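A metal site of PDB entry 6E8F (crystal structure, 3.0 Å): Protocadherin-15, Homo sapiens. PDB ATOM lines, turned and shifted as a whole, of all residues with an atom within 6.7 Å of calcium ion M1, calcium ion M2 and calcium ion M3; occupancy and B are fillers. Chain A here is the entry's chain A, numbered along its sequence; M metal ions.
Within 4 Å of calcium ion M1: Asn 249, Asn 251, Asp 281, Asp 283, Asn 287 and Asp 333.
Along chain A the residues within 4 Å of calcium ion M1 span positions 249 to 333.
The nearest printed residue that does not touch calcium ion M1 is Gly 288 (4.5 Å).
OD1 of Asp 216 binds calcium ion M3.
Calcium ion M3 is bound by the side-chain carboxylate (OE1) of Glu 145 (2.5 Å).
Calcium ion M3 is bound by OE1 of Glu 218, at 2.6 Å.
OD2 of Asp 250 binds calcium ion M3 (2.6 Å).
Calcium ion M3 has four donor atoms within binding distance.
Of the 27 residues printed, 7 come within 4 Å of calcium ion M2.
NE of Arg 341 is in hydrogen-bond range of O of Asn 249, at 2.7 Å.
The backbone carbonyl oxygen (O) of Glu 339 lies within hydrogen-bond range of the side-chain amide nitrogen (ND2) of Asn 249, 2.8 Å away.
The side-chain amide nitrogen (ND2) of Asn 251 sits close to the side-chain carboxylate (OD1) of Asp 250 (2.7 Å).
The side-chain carboxylate of Asp 333 sits at hydrogen-bond distance from the backbone NH of Arg 341, 3.0 Å away.
ND2 of Asn 287 lies within hydrogen-bond range of OD2 of Asp 247.
The guanidinium group (NE) of Arg 217 lies close to the side-chain carboxylate (OE2) of Glu 218, 2.8 Å away.
The guanidinium group (NE) of Arg 217 sits close to the side-chain carboxylate (OD1) of Asp 247, 2.9 Å away.
OD2 of Asp 247 sits at hydrogen-bond distance from N of Glu 284.
Four residues have an atom within 4 Å of calcium ion M3: Glu 145, Asp 216, Glu 218 and Asp 250.
OD1 of Asn 249 is bound to calcium ion M1 (2.1 Å).
Calcium ion M1 is bound by O of Asn 251, 2.2 Å away.
OD2 of Asp 333 is bound to calcium ion M1, 2.3 Å away.
OD2 of Asp 281 is bound to calcium ion M1 (2.3 Å).
Calcium ion M1 is bound by O of Asn 287 (2.3 Å).
Calcium ion M1 is bound by the side-chain carboxylate (OD2) of Asp 283 (2.4 Å).
Calcium ion M1 is bound by OD1 of Asp 281.
Calcium ion M1 has seven donor atoms within binding distance.
Calcium ion M2 is bound by the side-chain carboxylate (OE2) of Glu 145, the side-chain carboxylate (OE2) of Glu 218, the side-chain carboxylate (OD1) of Asp 247, the side-chain carboxylate (OD1) of Asp 283, the backbone carbonyl oxygen (O) of Ala 248, the side-chain carboxylate (OD1) of Asp 250 and the side-chain carboxylate (OE1) of Glu 218.
Calcium ion M2 has seven donor atoms within binding distance.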
ATOM      1  N   GLU A 145      23.065   2.562 -31.275  1.00  0.00           N
ATOM      2  CA  GLU A 145      23.247   3.269 -29.993  1.00  0.00           C
ATOM      3  C   GLU A 145      24.604   3.967 -30.009  1.00  0.00           C
ATOM      4  O   GLU A 145      24.789   4.951 -29.333  1.00  0.00           O
ATOM      5  CB  GLU A 145      23.096   2.383 -28.766  1.00  0.00           C
ATOM      6  CG  GLU A 145      24.069   1.223 -28.709  1.00  0.00           C
ATOM      7  CD  GLU A 145      23.953   0.384 -27.450  1.00  0.00           C
ATOM      8  OE1 GLU A 145      23.560   0.937 -26.407  1.00  0.00           O
ATOM      9  OE2 GLU A 145      24.278  -0.817 -27.497  1.00  0.00           O
ATOM     10  N   VAL A 215      21.879   7.935 -27.523  1.00  0.00           N
ATOM     11  CA  VAL A 215      20.823   7.049 -27.077  1.00  0.00           C
ATOM     12  C   VAL A 215      21.421   5.693 -26.695  1.00  0.00           C
ATOM     13  O   VAL A 215      22.268   5.156 -27.389  1.00  0.00           O
ATOM     14  CB  VAL A 215      19.738   6.895 -28.164  1.00  0.00           C
ATOM     15  CG1 VAL A 215      18.907   8.165 -28.295  1.00  0.00           C
ATOM     16  CG2 VAL A 215      20.318   6.465 -29.513  1.00  0.00           C
ATOM     17  N   ASP A 216      20.921   5.153 -25.591  1.00  0.00           N
ATOM     18  CA  ASP A 216      21.412   3.962 -24.995  1.00  0.00           C
ATOM     19  C   ASP A 216      20.370   2.866 -25.197  1.00  0.00           C
ATOM     20  O   ASP A 216      19.236   2.993 -24.715  1.00  0.00           O
ATOM     21  CB  ASP A 216      21.677   4.221 -23.512  1.00  0.00           C
ATOM     22  CG  ASP A 216      22.395   3.107 -22.775  1.00  0.00           C
ATOM     23  OD1 ASP A 216      22.544   1.996 -23.346  1.00  0.00           O
ATOM     24  OD2 ASP A 216      22.763   3.363 -21.612  1.00  0.00           O
ATOM     25  N   ARG A 217      20.740   1.794 -25.911  1.00  0.00           N
ATOM     26  CA  ARG A 217      19.772   0.714 -26.135  1.00  0.00           C
ATOM     27  C   ARG A 217      19.377   0.093 -24.792  1.00  0.00           C
ATOM     28  O   ARG A 217      18.279  -0.401 -24.620  1.00  0.00           O
ATOM     29  CB  ARG A 217      20.289  -0.391 -27.049  1.00  0.00           C
ATOM     30  CG  ARG A 217      19.206  -1.398 -27.422  1.00  0.00           C
ATOM     31  CD  ARG A 217      19.777  -2.779 -27.660  1.00  0.00           C
ATOM     32  NE  ARG A 217      20.286  -3.337 -26.425  1.00  0.00           N
ATOM     33  CZ  ARG A 217      19.549  -4.062 -25.583  1.00  0.00           C
ATOM     34  NH1 ARG A 217      18.250  -4.230 -25.831  1.00  0.00           N
ATOM     35  NH2 ARG A 217      20.109  -4.629 -24.528  1.00  0.00           N
ATOM     36  N   GLU A 218      20.303   0.125 -23.830  1.00  0.00           N
ATOM     37  CA  GLU A 218      20.075  -0.549 -22.574  1.00  0.00           C
ATOM     38  C   GLU A 218      19.082   0.261 -21.724  1.00  0.00           C
ATOM     39  O   GLU A 218      18.396  -0.330 -20.922  1.00  0.00           O
ATOM     40  CB  GLU A 218      21.404  -0.849 -21.889  1.00  0.00           C
ATOM     41  CG  GLU A 218      22.150  -2.024 -22.515  1.00  0.00           C
ATOM     42  CD  GLU A 218      22.709  -1.827 -23.925  1.00  0.00           C
ATOM     43  OE1 GLU A 218      23.384  -0.764 -24.199  1.00  0.00           O
ATOM     44  OE2 GLU A 218      22.475  -2.757 -24.759  1.00  0.00           O
ATOM     45  N   GLU A 219      18.977   1.593 -21.932  1.00  0.00           N
ATOM     46  CA  GLU A 219      17.851   2.379 -21.353  1.00  0.00           C
ATOM     47  C   GLU A 219      16.554   2.080 -22.098  1.00  0.00           C
ATOM     48  O   GLU A 219      15.738   1.275 -21.652  1.00  0.00           O
ATOM     49  CB  GLU A 219      18.101   3.885 -21.433  1.00  0.00           C
ATOM     50  CG  GLU A 219      18.762   4.476 -20.215  1.00  0.00           C
ATOM     51  CD  GLU A 219      19.420   5.810 -20.499  1.00  0.00           C
ATOM     52  OE1 GLU A 219      20.336   6.187 -19.738  1.00  0.00           O
ATOM     53  OE2 GLU A 219      19.027   6.471 -21.529  1.00  0.00           O
ATOM     54  N   MET A 246      19.507   0.107 -32.283  1.00  0.00           N
ATOM     55  CA  MET A 246      20.167  -1.162 -32.536  1.00  0.00           C
ATOM     56  C   MET A 246      21.379  -1.295 -31.615  1.00  0.00           C
ATOM     57  O   MET A 246      22.095  -0.307 -31.331  1.00  0.00           O
ATOM     58  CB  MET A 246      20.627  -1.259 -33.987  1.00  0.00           C
ATOM     59  CG  MET A 246      19.544  -0.924 -34.984  1.00  0.00           C
ATOM     60  SD  MET A 246      20.169  -0.982 -36.691  1.00  0.00           S
ATOM     61  CE  MET A 246      19.657  -2.636 -37.149  1.00  0.00           C
ATOM     62  N   ASP A 247      21.621  -2.544 -31.188  1.00  0.00           N
ATOM     63  CA  ASP A 247      22.616  -2.887 -30.197  1.00  0.00           C
ATOM     64  C   ASP A 247      24.014  -2.691 -30.771  1.00  0.00           C
ATOM     65  O   ASP A 247      24.245  -2.861 -31.965  1.00  0.00           O
ATOM     66  CB  ASP A 247      22.442  -4.326 -29.727  1.00  0.00           C
ATOM     67  CG  ASP A 247      23.226  -4.646 -28.459  1.00  0.00           C
ATOM     68  OD1 ASP A 247      22.957  -4.017 -27.410  1.00  0.00           O
ATOM     69  OD2 ASP A 247      24.097  -5.521 -28.536  1.00  0.00           O
ATOM     70  N   ALA A 248      24.927  -2.272 -29.891  1.00  0.00           N
ATOM     71  CA  ALA A 248      26.344  -2.332 -30.054  1.00  0.00           C
ATOM     72  C   ALA A 248      26.899  -3.063 -28.840  1.00  0.00           C
ATOM     73  O   ALA A 248      26.217  -3.137 -27.801  1.00  0.00           O
ATOM     74  CB  ALA A 248      26.887  -0.940 -30.145  1.00  0.00           C
ATOM     75  N   ASN A 249      28.125  -3.595 -28.954  1.00  0.00           N
ATOM     76  CA  ASN A 249      28.777  -4.290 -27.856  1.00  0.00           C
ATOM     77  C   ASN A 249      29.497  -3.258 -26.978  1.00  0.00           C
ATOM     78  O   ASN A 249      30.728  -3.153 -27.022  1.00  0.00           O
ATOM     79  CB  ASN A 249      29.706  -5.406 -28.317  1.00  0.00           C
ATOM     80  CG  ASN A 249      30.037  -6.359 -27.183  1.00  0.00           C
ATOM     81  OD1 ASN A 249      29.227  -6.529 -26.276  1.00  0.00           O
ATOM     82  ND2 ASN A 249      31.201  -6.981 -27.218  1.00  0.00           N
ATOM     83  N   ASP A 250      28.719  -2.527 -26.168  1.00  0.00           N
ATOM     84  CA  ASP A 250      29.241  -1.514 -25.241  1.00  0.00           C
ATOM     85  C   ASP A 250      29.175  -2.000 -23.790  1.00  0.00           C
ATOM     86  O   ASP A 250      29.299  -1.209 -22.855  1.00  0.00           O
ATOM     87  CB  ASP A 250      28.532  -0.161 -25.402  1.00  0.00           C
ATOM     88  CG  ASP A 250      27.007  -0.168 -25.546  1.00  0.00           C
ATOM     89  OD1 ASP A 250      26.364  -1.160 -25.134  1.00  0.00           O
ATOM     90  OD2 ASP A 250      26.478   0.842 -26.055  1.00  0.00           O
ATOM     91  N   ASN A 251      28.975  -3.311 -23.563  1.00  0.00           N
ATOM     92  CA  ASN A 251      28.873  -3.818 -22.211  1.00  0.00           C
ATOM     93  C   ASN A 251      29.719  -5.084 -22.061  1.00  0.00           C
ATOM     94  O   ASN A 251      29.527  -6.073 -22.779  1.00  0.00           O
ATOM     95  CB  ASN A 251      27.417  -4.051 -21.817  1.00  0.00           C
ATOM     96  CG  ASN A 251      26.699  -2.737 -21.590  1.00  0.00           C
ATOM     97  OD1 ASN A 251      26.746  -2.195 -20.481  1.00  0.00           O
ATOM     98  ND2 ASN A 251      26.077  -2.203 -22.630  1.00  0.00           N
ATOM     99  N   THR A 252      30.657  -5.004 -21.107  1.00  0.00           N
ATOM    100  CA  THR A 252      31.590  -6.071 -20.810  1.00  0.00           C
ATOM    101  C   THR A 252      30.884  -7.085 -19.908  1.00  0.00           C
ATOM    102  O   THR A 252      30.060  -6.705 -19.075  1.00  0.00           O
ATOM    103  CB  THR A 252      32.842  -5.506 -20.142  1.00  0.00           C
ATOM    104  OG1 THR A 252      33.395  -4.474 -20.963  1.00  0.00           O
ATOM    105  CG2 THR A 252      33.898  -6.571 -19.930  1.00  0.00           C
ATOM    106  N   PRO A 253      31.145  -8.403 -20.067  1.00  0.00           N
ATOM    107  CA  PRO A 253      30.609  -9.403 -19.137  1.00  0.00           C
ATOM    108  C   PRO A 253      31.389  -9.184 -17.842  1.00  0.00           C
ATOM    109  O   PRO A 253      32.565  -9.456 -17.829  1.00  0.00           O
ATOM    110  CB  PRO A 253      30.871 -10.769 -19.781  1.00  0.00           C
ATOM    111  CG  PRO A 253      31.297 -10.435 -21.208  1.00  0.00           C
ATOM    112  CD  PRO A 253      31.887  -9.041 -21.164  1.00  0.00           C
ATOM    113  N   ASP A 281      26.023  -9.510 -18.798  1.00  0.00           N
ATOM    114  CA  ASP A 281      26.308  -8.660 -19.941  1.00  0.00           C
ATOM    115  C   ASP A 281      24.969  -8.114 -20.395  1.00  0.00           C
ATOM    116  O   ASP A 281      24.180  -8.865 -20.957  1.00  0.00           O
ATOM    117  CB  ASP A 281      26.966  -9.423 -21.095  1.00  0.00           C
ATOM    118  CG  ASP A 281      27.543  -8.543 -22.197  1.00  0.00           C
ATOM    119  OD1 ASP A 281      26.920  -7.512 -22.542  1.00  0.00           O
ATOM    120  OD2 ASP A 281      28.615  -8.896 -22.720  1.00  0.00           O
ATOM    121  N   ALA A 282      24.747  -6.819 -20.167  1.00  0.00           N
ATOM    122  CA  ALA A 282      23.449  -6.176 -20.416  1.00  0.00           C
ATOM    123  C   ALA A 282      23.097  -6.130 -21.916  1.00  0.00           C
ATOM    124  O   ALA A 282      21.955  -5.908 -22.254  1.00  0.00           O
ATOM    125  CB  ALA A 282      23.463  -4.792 -19.827  1.00  0.00           C
ATOM    126  N   ASP A 283      24.081  -6.339 -22.812  1.00  0.00           N
ATOM    127  CA  ASP A 283      23.874  -6.273 -24.259  1.00  0.00           C
ATOM    128  C   ASP A 283      22.797  -7.266 -24.714  1.00  0.00           C
ATOM    129  O   ASP A 283      22.351  -8.126 -23.954  1.00  0.00           O
ATOM    130  CB  ASP A 283      25.188  -6.476 -25.000  1.00  0.00           C
ATOM    131  CG  ASP A 283      26.146  -5.293 -24.888  1.00  0.00           C
ATOM    132  OD1 ASP A 283      25.644  -4.148 -24.776  1.00  0.00           O
ATOM    133  OD2 ASP A 283      27.376  -5.529 -24.911  1.00  0.00           O
ATOM    134  N   GLU A 284      22.395  -7.098 -25.976  1.00  0.00           N
ATOM    135  CA  GLU A 284      21.328  -7.850 -26.629  1.00  0.00           C
ATOM    136  C   GLU A 284      21.965  -8.891 -27.542  1.00  0.00           C
ATOM    137  O   GLU A 284      23.103  -8.738 -28.031  1.00  0.00           O
ATOM    138  CB  GLU A 284      20.419  -6.895 -27.429  1.00  0.00           C
ATOM    139  CG  GLU A 284      19.636  -7.542 -28.583  1.00  0.00           C
ATOM    140  CD  GLU A 284      18.691  -6.636 -29.371  1.00  0.00           C
ATOM    141  OE1 GLU A 284      19.178  -5.752 -30.105  1.00  0.00           O
ATOM    142  OE2 GLU A 284      17.462  -6.833 -29.258  1.00  0.00           O
ATOM    143  N   SER A 286      23.791 -11.795 -29.277  1.00  0.00           N
ATOM    144  CA  SER A 286      25.018 -12.508 -28.914  1.00  0.00           C
ATOM    145  C   SER A 286      26.093 -11.536 -28.384  1.00  0.00           C
ATOM    146  O   SER A 286      27.099 -11.946 -27.856  1.00  0.00           O
ATOM    147  CB  SER A 286      25.500 -13.344 -30.059  1.00  0.00           C
ATOM    148  OG  SER A 286      26.269 -12.554 -30.928  1.00  0.00           O
ATOM    149  N   ASN A 287      25.831 -10.225 -28.448  1.00  0.00           N
ATOM    150  CA  ASN A 287      26.691  -9.240 -27.790  1.00  0.00           C
ATOM    151  C   ASN A 287      26.600  -9.372 -26.270  1.00  0.00           C
ATOM    152  O   ASN A 287      27.483  -8.856 -25.550  1.00  0.00           O
ATOM    153  CB  ASN A 287      26.322  -7.813 -28.183  1.00  0.00           C
ATOM    154  CG  ASN A 287      26.591  -7.525 -29.643  1.00  0.00           C
ATOM    155  OD1 ASN A 287      26.600  -8.437 -30.461  1.00  0.00           O
ATOM    156  ND2 ASN A 287      26.841  -6.272 -29.965  1.00  0.00           N
ATOM    157  N   GLY A 288      25.529 -10.021 -25.787  1.00  0.00           N
ATOM    158  CA  GLY A 288      25.263 -10.214 -24.368  1.00  0.00           C
ATOM    159  C   GLY A 288      25.261 -11.674 -23.968  1.00  0.00           C
ATOM    160  O   GLY A 288      24.960 -11.994 -22.823  1.00  0.00           O
ATOM    161  N   GLU A 289      25.602 -12.548 -24.918  1.00  0.00           N
ATOM    162  CA  GLU A 289      25.784 -13.991 -24.716  1.00  0.00           C
ATOM    163  C   GLU A 289      27.184 -14.202 -24.134  1.00  0.00           C
ATOM    164  O   GLU A 289      28.135 -13.644 -24.650  1.00  0.00           O
ATOM    165  CB  GLU A 289      25.604 -14.676 -26.073  1.00  0.00           C
ATOM    166  CG  GLU A 289      25.121 -16.111 -26.044  1.00  0.00           C
ATOM    167  CD  GLU A 289      25.615 -16.890 -27.262  1.00  0.00           C
ATOM    168  OE1 GLU A 289      26.811 -17.255 -27.270  1.00  0.00           O
ATOM    169  OE2 GLU A 289      24.844 -17.060 -28.226  1.00  0.00           O
ATOM    170  N   ASP A 333      31.903 -12.131 -24.107  1.00  0.00           N
ATOM    171  CA  ASP A 333      30.665 -12.150 -24.904  1.00  0.00           C
ATOM    172  C   ASP A 333      30.965 -12.748 -26.279  1.00  0.00           C
ATOM    173  O   ASP A 333      32.140 -12.869 -26.646  1.00  0.00           O
ATOM    174  CB  ASP A 333      30.026 -10.758 -24.980  1.00  0.00           C
ATOM    175  CG  ASP A 333      30.902  -9.644 -25.533  1.00  0.00           C
ATOM    176  OD1 ASP A 333      31.808  -9.928 -26.355  1.00  0.00           O
ATOM    177  OD2 ASP A 333      30.668  -8.481 -25.164  1.00  0.00           O
ATOM    178  N   ASN A 334      29.925 -13.118 -27.035  1.00  0.00           N
ATOM    179  CA  ASN A 334      30.074 -13.741 -28.361  1.00  0.00           C
ATOM    180  C   ASN A 334      29.856 -12.713 -29.480  1.00  0.00           C
ATOM    181  O   ASN A 334      29.244 -13.026 -30.495  1.00  0.00           O
ATOM    182  CB  ASN A 334      29.190 -14.982 -28.528  1.00  0.00           C
ATOM    183  CG  ASN A 334      29.602 -16.113 -27.594  1.00  0.00           C
ATOM    184  OD1 ASN A 334      30.041 -15.862 -26.478  1.00  0.00           O
ATOM    185  ND2 ASN A 334      29.490 -17.352 -28.048  1.00  0.00           N
ATOM    186  N   ALA A 335      30.414 -11.513 -29.319  1.00  0.00           N
ATOM    187  CA  ALA A 335      30.468 -10.553 -30.431  1.00  0.00           C
ATOM    188  C   ALA A 335      31.465 -11.073 -31.455  1.00  0.00           C
ATOM    189  O   ALA A 335      32.189 -12.028 -31.188  1.00  0.00           O
ATOM    190  CB  ALA A 335      30.858  -9.185 -29.931  1.00  0.00           C
ATOM    191  N   GLU A 339      35.299  -6.813 -31.969  1.00  0.00           N
ATOM    192  CA  GLU A 339      34.428  -5.948 -31.139  1.00  0.00           C
ATOM    193  C   GLU A 339      34.061  -6.638 -29.807  1.00  0.00           C
ATOM    194  O   GLU A 339      33.180  -6.148 -29.087  1.00  0.00           O
ATOM    195  CB  GLU A 339      33.117  -5.660 -31.890  1.00  0.00           C
ATOM    196  CG  GLU A 339      33.316  -5.035 -33.259  1.00  0.00           C
ATOM    197  CD  GLU A 339      32.346  -5.555 -34.318  1.00  0.00           C
ATOM    198  OE1 GLU A 339      31.223  -5.970 -33.943  1.00  0.00           O
ATOM    199  OE2 GLU A 339      32.725  -5.583 -35.511  1.00  0.00           O
ATOM    200  N   ARG A 341      34.316  -8.340 -25.959  1.00  0.00           N
ATOM    201  CA  ARG A 341      34.818  -7.873 -24.678  1.00  0.00           C
ATOM    202  C   ARG A 341      34.821  -9.015 -23.675  1.00  0.00           C
ATOM    203  O   ARG A 341      34.109 -10.002 -23.845  1.00  0.00           O
ATOM    204  CB  ARG A 341      33.974  -6.733 -24.126  1.00  0.00           C
ATOM    205  CG  ARG A 341      34.144  -5.431 -24.888  1.00  0.00           C
ATOM    206  CD  ARG A 341      32.813  -4.806 -25.267  1.00  0.00           C
ATOM    207  NE  ARG A 341      33.009  -3.388 -25.521  1.00  0.00           N
ATOM    208  CZ  ARG A 341      33.219  -2.488 -24.571  1.00  0.00           C
ATOM    209  NH1 ARG A 341      33.184  -2.863 -23.305  1.00  0.00           N
ATOM    210  NH2 ARG A 341      33.465  -1.248 -24.898  1.00  0.00           N
HETATM  211 CA    CA M   1      28.842  -7.379 -24.422  1.00  0.00          CA
HETATM  212 CA    CA M   2      24.337  -2.551 -26.147  1.00  0.00          CA
HETATM  213 CA    CA M   3      24.732   1.409 -24.263  1.00  0.00          CA
